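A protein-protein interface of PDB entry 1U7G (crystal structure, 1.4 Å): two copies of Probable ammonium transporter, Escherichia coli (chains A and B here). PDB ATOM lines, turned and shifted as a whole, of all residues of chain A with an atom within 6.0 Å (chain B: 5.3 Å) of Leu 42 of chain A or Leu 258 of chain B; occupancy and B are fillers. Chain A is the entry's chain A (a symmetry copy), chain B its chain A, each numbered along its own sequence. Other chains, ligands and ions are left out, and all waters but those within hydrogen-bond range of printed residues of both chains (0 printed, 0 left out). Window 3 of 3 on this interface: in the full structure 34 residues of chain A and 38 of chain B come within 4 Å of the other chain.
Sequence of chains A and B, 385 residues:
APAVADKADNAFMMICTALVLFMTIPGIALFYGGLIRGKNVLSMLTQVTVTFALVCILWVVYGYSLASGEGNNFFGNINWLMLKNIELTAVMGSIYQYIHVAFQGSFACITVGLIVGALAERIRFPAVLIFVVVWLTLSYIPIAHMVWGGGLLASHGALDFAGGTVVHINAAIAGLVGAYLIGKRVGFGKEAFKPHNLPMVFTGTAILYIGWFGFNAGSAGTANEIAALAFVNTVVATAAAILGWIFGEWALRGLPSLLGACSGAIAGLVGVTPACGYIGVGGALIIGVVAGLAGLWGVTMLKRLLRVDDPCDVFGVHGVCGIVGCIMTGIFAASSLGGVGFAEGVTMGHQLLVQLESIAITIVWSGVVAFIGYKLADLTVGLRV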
ATOM      1  N   ILE A  36      -2.422   4.176   2.787  1.00  0.00           N
ATOM      2  CA  ILE A  36      -1.387   3.188   2.514  1.00  0.00           C
ATOM      3  C   ILE A  36      -0.050   3.731   3.009  1.00  0.00           C
ATOM      4  O   ILE A  36       0.202   4.905   3.331  1.00  0.00           O
ATOM      5  CB  ILE A  36      -1.380   2.892   1.017  1.00  0.00           C
ATOM      6  CG1 ILE A  36      -0.931   4.136   0.237  1.00  0.00           C
ATOM      7  CG2 ILE A  36      -2.699   2.389   0.444  1.00  0.00           C
ATOM      8  CD1 ILE A  36      -0.882   3.738  -1.239  1.00  0.00           C
ATOM      9  N   GLY A  38       3.821   4.797   3.019  1.00  0.00           N
ATOM     10  CA  GLY A  38       4.586   5.771   2.256  1.00  0.00           C
ATOM     11  C   GLY A  38       5.184   5.052   1.057  1.00  0.00           C
ATOM     12  O   GLY A  38       5.119   5.648  -0.022  1.00  0.00           O
ATOM     13  N   LYS A  39       5.712   3.853   1.280  1.00  0.00           N
ATOM     14  CA  LYS A  39       6.511   3.206   0.231  1.00  0.00           C
ATOM     15  C   LYS A  39       5.710   2.802  -0.990  1.00  0.00           C
ATOM     16  O   LYS A  39       6.318   2.514  -2.018  1.00  0.00           O
ATOM     17  CB  LYS A  39       7.238   1.986   0.790  1.00  0.00           C
ATOM     18  CG  LYS A  39       6.466   0.675   0.740  1.00  0.00           C
ATOM     19  CD  LYS A  39       7.351  -0.439   1.318  1.00  0.00           C
ATOM     20  CE  LYS A  39       7.138  -1.759   0.594  1.00  0.00           C
ATOM     21  NZ  LYS A  39       8.355  -2.633   0.640  1.00  0.00           N
ATOM     22  N   ASN A  40       4.387   2.766  -0.924  1.00  0.00           N
ATOM     23  CA  ASN A  40       3.544   2.331  -2.013  1.00  0.00           C
ATOM     24  C   ASN A  40       2.724   3.503  -2.589  1.00  0.00           C
ATOM     25  O   ASN A  40       1.963   3.306  -3.531  1.00  0.00           O
ATOM     26  CB  ASN A  40       2.578   1.258  -1.489  1.00  0.00           C
ATOM     27  CG  ASN A  40       3.278  -0.064  -1.246  1.00  0.00           C
ATOM     28  OD1 ASN A  40       4.368  -0.303  -1.763  1.00  0.00           O
ATOM     29  ND2 ASN A  40       2.620  -0.893  -0.431  1.00  0.00           N
ATOM     30  N   VAL A  41       2.890   4.687  -2.016  1.00  0.00           N
ATOM     31  CA  VAL A  41       2.007   5.747  -2.428  1.00  0.00           C
ATOM     32  C   VAL A  41       2.293   6.141  -3.873  1.00  0.00           C
ATOM     33  O   VAL A  41       1.369   6.384  -4.644  1.00  0.00           O
ATOM     34  CB  VAL A  41       2.186   6.976  -1.525  1.00  0.00           C
ATOM     35  CG1 VAL A  41       1.531   8.181  -2.188  1.00  0.00           C
ATOM     36  CG2 VAL A  41       1.580   6.689  -0.174  1.00  0.00           C
ATOM     37  N   LEU A  42       3.562   6.200  -4.202  1.00  0.00           N
ATOM     38  CA  LEU A  42       3.952   6.547  -5.569  1.00  0.00           C
ATOM     39  C   LEU A  42       3.344   5.642  -6.633  1.00  0.00           C
ATOM     40  O   LEU A  42       2.800   6.101  -7.652  1.00  0.00           O
ATOM     41  CB  LEU A  42       5.454   6.687  -5.776  1.00  0.00           C
ATOM     42  CG  LEU A  42       6.044   7.832  -4.958  1.00  0.00           C
ATOM     43  CD1 LEU A  42       7.504   7.955  -5.373  1.00  0.00           C
ATOM     44  CD2 LEU A  42       5.329   9.159  -5.114  1.00  0.00           C
ATOM     45  N   SER A  43       3.444   4.351  -6.388  1.00  0.00           N
ATOM     46  CA  SER A  43       2.887   3.356  -7.234  1.00  0.00           C
ATOM     47  C   SER A  43       1.368   3.517  -7.343  1.00  0.00           C
ATOM     48  O   SER A  43       0.844   3.430  -8.438  1.00  0.00           O
ATOM     49  CB  SER A  43       3.235   1.963  -6.688  1.00  0.00           C
ATOM     50  OG  SER A  43       2.672   1.020  -7.574  1.00  0.00           O
ATOM     51  N   MET A  44       0.739   3.731  -6.196  1.00  0.00           N
ATOM     52  CA  MET A  44      -0.711   3.837  -6.233  1.00  0.00           C
ATOM     53  C   MET A  44      -1.103   5.068  -7.051  1.00  0.00           C
ATOM     54  O   MET A  44      -2.041   4.956  -7.849  1.00  0.00           O
ATOM     55  CB  MET A  44      -1.279   3.956  -4.810  1.00  0.00           C
ATOM     56  CG  MET A  44      -2.782   4.168  -4.766  1.00  0.00           C
ATOM     57  SD  MET A  44      -3.312   5.926  -4.843  1.00  0.00           S
ATOM     58  CE  MET A  44      -2.415   6.581  -3.373  1.00  0.00           C
ATOM     59  N   LEU A  45      -0.381   6.178  -6.842  1.00  0.00           N
ATOM     60  CA  LEU A  45      -0.789   7.381  -7.546  1.00  0.00           C
ATOM     61  C   LEU A  45      -0.595   7.177  -9.034  1.00  0.00           C
ATOM     62  O   LEU A  45      -1.367   7.623  -9.856  1.00  0.00           O
ATOM     63  CB  LEU A  45       0.008   8.596  -7.146  1.00  0.00           C
ATOM     64  CG  LEU A  45      -0.236   9.005  -5.694  1.00  0.00           C
ATOM     65  CD1 LEU A  45       0.612  10.153  -5.222  1.00  0.00           C
ATOM     66  CD2 LEU A  45      -1.719   9.428  -5.455  1.00  0.00           C
ATOM     67  N   THR A  46       0.483   6.470  -9.396  1.00  0.00           N
ATOM     68  CA  THR A  46       0.710   6.201 -10.829  1.00  0.00           C
ATOM     69  C   THR A  46      -0.389   5.342 -11.392  1.00  0.00           C
ATOM     70  O   THR A  46      -0.895   5.590 -12.482  1.00  0.00           O
ATOM     71  CB  THR A  46       2.084   5.501 -11.004  1.00  0.00           C
ATOM     72  OG1 THR A  46       3.071   6.270 -10.319  1.00  0.00           O
ATOM     73  CG2 THR A  46       2.462   5.422 -12.467  1.00  0.00           C
ATOM     74  N   GLN A  47      -0.774   4.287 -10.650  1.00  0.00           N
ATOM     75  CA  GLN A  47      -1.810   3.396 -11.158  1.00  0.00           C
ATOM     76  C   GLN A  47      -3.136   4.133 -11.231  1.00  0.00           C
ATOM     77  O   GLN A  47      -3.890   3.901 -12.165  1.00  0.00           O
ATOM     78  CB  GLN A  47      -1.990   2.152 -10.288  1.00  0.00           C
ATOM     79  CG  GLN A  47      -0.806   1.171 -10.530  1.00  0.00           C
ATOM     80  CD  GLN A  47      -1.132  -0.163  -9.903  1.00  0.00           C
ATOM     81  OE1 GLN A  47      -2.310  -0.480  -9.618  1.00  0.00           O
ATOM     82  NE2 GLN A  47      -0.109  -0.935  -9.686  1.00  0.00           N
ATOM     83  N   THR A  49      -3.594   7.266 -11.760  1.00  0.00           N
ATOM     84  CA  THR A  49      -3.572   8.274 -12.826  1.00  0.00           C
ATOM     85  C   THR A  49      -3.627   7.562 -14.173  1.00  0.00           C
ATOM     86  O   THR A  49      -4.302   7.977 -15.094  1.00  0.00           O
ATOM     87  CB  THR A  49      -2.267   9.091 -12.740  1.00  0.00           C
ATOM     88  OG1 THR A  49      -2.208   9.732 -11.470  1.00  0.00           O
ATOM     89  CG2 THR A  49      -2.208  10.151 -13.833  1.00  0.00           C
ATOM     90  N   PRO B 195      11.528  11.770  -4.402  1.00  0.00           N
ATOM     91  CA  PRO B 195      10.271  11.022  -4.508  1.00  0.00           C
ATOM     92  C   PRO B 195       9.302  11.386  -3.395  1.00  0.00           C
ATOM     93  O   PRO B 195       8.115  11.429  -3.649  1.00  0.00           O
ATOM     94  CB  PRO B 195      10.724   9.581  -4.396  1.00  0.00           C
ATOM     95  CG  PRO B 195      12.155   9.621  -4.903  1.00  0.00           C
ATOM     96  CD  PRO B 195      12.730  10.914  -4.380  1.00  0.00           C
ATOM     97  N   LEU B 198       6.869  13.996  -4.454  1.00  0.00           N
ATOM     98  CA  LEU B 198       6.089  13.838  -5.691  1.00  0.00           C
ATOM     99  C   LEU B 198       4.602  13.726  -5.424  1.00  0.00           C
ATOM    100  O   LEU B 198       3.886  14.115  -6.380  1.00  0.00           O
ATOM    101  CB  LEU B 198       6.644  12.626  -6.476  1.00  0.00           C
ATOM    102  CG  LEU B 198       8.098  12.847  -6.963  1.00  0.00           C
ATOM    103  CD1 LEU B 198       8.578  11.609  -7.683  1.00  0.00           C
ATOM    104  CD2 LEU B 198       8.219  14.102  -7.843  1.00  0.00           C
ATOM    105  N   PRO B 199       4.030  13.274  -4.332  1.00  0.00           N
ATOM    106  CA  PRO B 199       2.567  13.406  -4.177  1.00  0.00           C
ATOM    107  C   PRO B 199       2.087  14.844  -4.312  1.00  0.00           C
ATOM    108  O   PRO B 199       0.938  15.042  -4.742  1.00  0.00           O
ATOM    109  CB  PRO B 199       2.308  12.859  -2.781  1.00  0.00           C
ATOM    110  CG  PRO B 199       3.390  11.817  -2.668  1.00  0.00           C
ATOM    111  CD  PRO B 199       4.625  12.521  -3.167  1.00  0.00           C
ATOM    112  N   PHE B 202       1.765  15.420  -7.931  1.00  0.00           N
ATOM    113  CA  PHE B 202       0.486  14.834  -8.350  1.00  0.00           C
ATOM    114  C   PHE B 202      -0.651  15.755  -7.975  1.00  0.00           C
ATOM    115  O   PHE B 202      -1.563  15.968  -8.790  1.00  0.00           O
ATOM    116  CB  PHE B 202       0.309  13.450  -7.690  1.00  0.00           C
ATOM    117  CG  PHE B 202      -1.097  12.932  -7.899  1.00  0.00           C
ATOM    118  CD1 PHE B 202      -1.449  12.365  -9.115  1.00  0.00           C
ATOM    119  CD2 PHE B 202      -2.053  13.029  -6.905  1.00  0.00           C
ATOM    120  CE1 PHE B 202      -2.774  11.928  -9.275  1.00  0.00           C
ATOM    121  CE2 PHE B 202      -3.353  12.611  -7.041  1.00  0.00           C
ATOM    122  CZ  PHE B 202      -3.714  12.043  -8.261  1.00  0.00           C
ATOM    123  N   PRO B 256       6.760   2.643 -15.810  1.00  0.00           N
ATOM    124  CA  PRO B 256       6.139   3.959 -15.758  1.00  0.00           C
ATOM    125  C   PRO B 256       6.570   4.661 -14.477  1.00  0.00           C
ATOM    126  O   PRO B 256       6.997   3.970 -13.541  1.00  0.00           O
ATOM    127  CB  PRO B 256       4.647   3.609 -15.695  1.00  0.00           C
ATOM    128  CG  PRO B 256       4.650   2.321 -14.948  1.00  0.00           C
ATOM    129  CD  PRO B 256       5.823   1.563 -15.509  1.00  0.00           C
ATOM    130  N   SER B 257       6.428   5.985 -14.380  1.00  0.00           N
ATOM    131  CA  SER B 257       6.627   6.630 -13.092  1.00  0.00           C
ATOM    132  C   SER B 257       5.519   7.626 -12.829  1.00  0.00           C
ATOM    133  O   SER B 257       4.838   8.066 -13.758  1.00  0.00           O
ATOM    134  CB  SER B 257       7.941   7.393 -13.131  1.00  0.00           C
ATOM    135  OG  SER B 257       7.906   8.500 -14.029  1.00  0.00           O
ATOM    136  N   LEU B 258       5.378   7.990 -11.570  1.00  0.00           N
ATOM    137  CA  LEU B 258       4.364   8.997 -11.228  1.00  0.00           C
ATOM    138  C   LEU B 258       4.687  10.281 -11.938  1.00  0.00           C
ATOM    139  O   LEU B 258       3.818  10.940 -12.499  1.00  0.00           O
ATOM    140  CB  LEU B 258       4.311   9.193  -9.701  1.00  0.00           C
ATOM    141  CG  LEU B 258       3.362  10.361  -9.359  1.00  0.00           C
ATOM    142  CD1 LEU B 258       1.925  10.012  -9.772  1.00  0.00           C
ATOM    143  CD2 LEU B 258       3.572  10.763  -7.936  1.00  0.00           C
ATOM    144  N   LEU B 259       5.955  10.712 -11.933  1.00  0.00           N
ATOM    145  CA  LEU B 259       6.239  11.957 -12.595  1.00  0.00           C
ATOM    146  C   LEU B 259       5.944  11.845 -14.097  1.00  0.00           C
ATOM    147  O   LEU B 259       5.530  12.851 -14.694  1.00  0.00           O
ATOM    148  CB  LEU B 259       7.672  12.397 -12.323  1.00  0.00           C
ATOM    149  CG  LEU B 259       8.003  13.804 -12.818  1.00  0.00           C
ATOM    150  CD1 LEU B 259       6.887  14.788 -12.491  1.00  0.00           C
ATOM    151  CD2 LEU B 259       9.321  14.223 -12.209  1.00  0.00           C
ATOM    152  N   GLY B 260       6.176  10.640 -14.625  1.00  0.00           N
ATOM    153  CA  GLY B 260       5.886  10.486 -16.056  1.00  0.00           C
ATOM    154  C   GLY B 260       4.386  10.649 -16.295  1.00  0.00           C
ATOM    155  O   GLY B 260       3.930  11.307 -17.237  1.00  0.00           O
ATOM    156  N   ALA B 261       3.591  10.060 -15.423  1.00  0.00           N
ATOM    157  CA  ALA B 261       2.141  10.144 -15.593  1.00  0.00           C
ATOM    158  C   ALA B 261       1.686  11.586 -15.476  1.00  0.00           C
ATOM    159  O   ALA B 261       0.857  12.056 -16.250  1.00  0.00           O
ATOM    160  CB  ALA B 261       1.436   9.262 -14.561  1.00  0.00           C
ATOM    161  N   CYS B 262       2.164  12.292 -14.461  1.00  0.00           N
ATOM    162  CA  CYS B 262       1.750  13.671 -14.288  1.00  0.00           C
ATOM    163  C   CYS B 262       2.228  14.538 -15.461  1.00  0.00           C
ATOM    164  O   CYS B 262       1.492  15.399 -15.935  1.00  0.00           O
ATOM    165  CB  CYS B 262       2.357  14.252 -13.010  1.00  0.00           C
ATOM    166  SG  CYS B 262       1.655  13.461 -11.538  1.00  0.00           S
ATOM    167  N   SER B 263       3.477  14.295 -15.917  1.00  0.00           N
ATOM    168  CA  SER B 263       3.986  15.074 -17.015  1.00  0.00           C
ATOM    169  C   SER B 263       3.176  14.823 -18.275  1.00  0.00           C
ATOM    170  O   SER B 263       2.908  15.745 -19.036  1.00  0.00           O
ATOM    171  CB  SER B 263       5.470  14.659 -17.251  1.00  0.00           C
ATOM    172  OG  SER B 263       6.192  14.995 -16.061  1.00  0.00           O
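The side-chain hydroxyl of Thr 46 of chain A lies within hydrogen-bond range of the backbone NH of Leu 258 of chain B (3.1 Å).
The side-chain hydroxyl (OG) of Ser 257 of chain B lies within hydrogen-bond range of the backbone NH (N) of Gly 260 of chain B (2.8 Å). The side-chain sulfur of Cys 262 of chain B sits at hydrogen-bond distance from the backbone carbonyl oxygen of Leu 258 of chain B. OG1 of Thr 46 of chain A lies within hydrogen-bond range of O of Leu 42 of chain A, at 2.7 Å. The backbone carbonyl oxygen (O) of Leu 45 of chain A is in hydrogen-bond range of the side-chain hydroxyl (OG1) of Thr 49 of chain A, 2.8 Å away.
Among the printed residues, merely in contact across the chains: Leu 42 of chain A with Pro 195 of chain B (3.7 Å), Leu 42 of chain A with Leu 198 of chain B (3.95 Å), Leu 42 of chain A with Pro 199 of chain B (3.9 Å), Leu 42 of chain A with Leu 258 of chain B (3.7 Å), Leu 45 of chain A with Pro 199 of chain B (3.9 Å), Leu 45 of chain A with Phe 202 of chain B (3.9 Å), Leu 45 of chain A with Leu 258 of chain B (3.5 Å), Thr 46 of chain A with Ser 257 of chain B (3.8 Å), Thr 49 of chain A with Phe 202 of chain B (3.2 Å) and Thr 49 of chain A with Ala 261 of chain B (3.8 Å).
Of chain B, only Pro 195, Leu 198, Pro 199 and Leu 258 come within 4 Å of Leu 42 of chain A. Printed residues of chain A within 4 Å of Ala 261 of chain B: Thr 49. Of the printed residues of chain A, Pro 199 of chain B touches Leu 42 (3.9 Å) and Leu 45 (3.9 Å). Printed residues of chain A within 4 Å of Ser 257 of chain B: Thr 46 (3.8 Å). Of the printed residues of chain A, Leu 198 of chain B touches Leu 42. Printed residues of chain A within 4 Å of Pro 195 of chain B: Leu 42 (3.7 Å). Lys 39 of chain A touches none of the printed residues of chain B.
Of the 12 printed residues of chain A, 4 touch a printed residue of chain B. Of the 12 printed residues of chain B, 7 touch a printed residue of chain A. Printed residues of chain B that touch a printed residue of chain A: Pro 195, Leu 198, Pro 199, Phe 202, Ser 257, Leu 258 and Ala 261. Hydrophobic or aromatic side chains of chain B within 4 Å of the printed part of chain A: Pro 195, Leu 198, Pro 199, Phe 202, Leu 258 and Ala 261. Among the printed residues, no Asp or Glu carboxylate lies within 4 Å of a Lys or Arg side-chain nitrogen of the other chain.
No position is printed for both chains. Of the 11 pairs that touch across the chains among the printed residues, none has its exchanged pair printed and touching as well.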
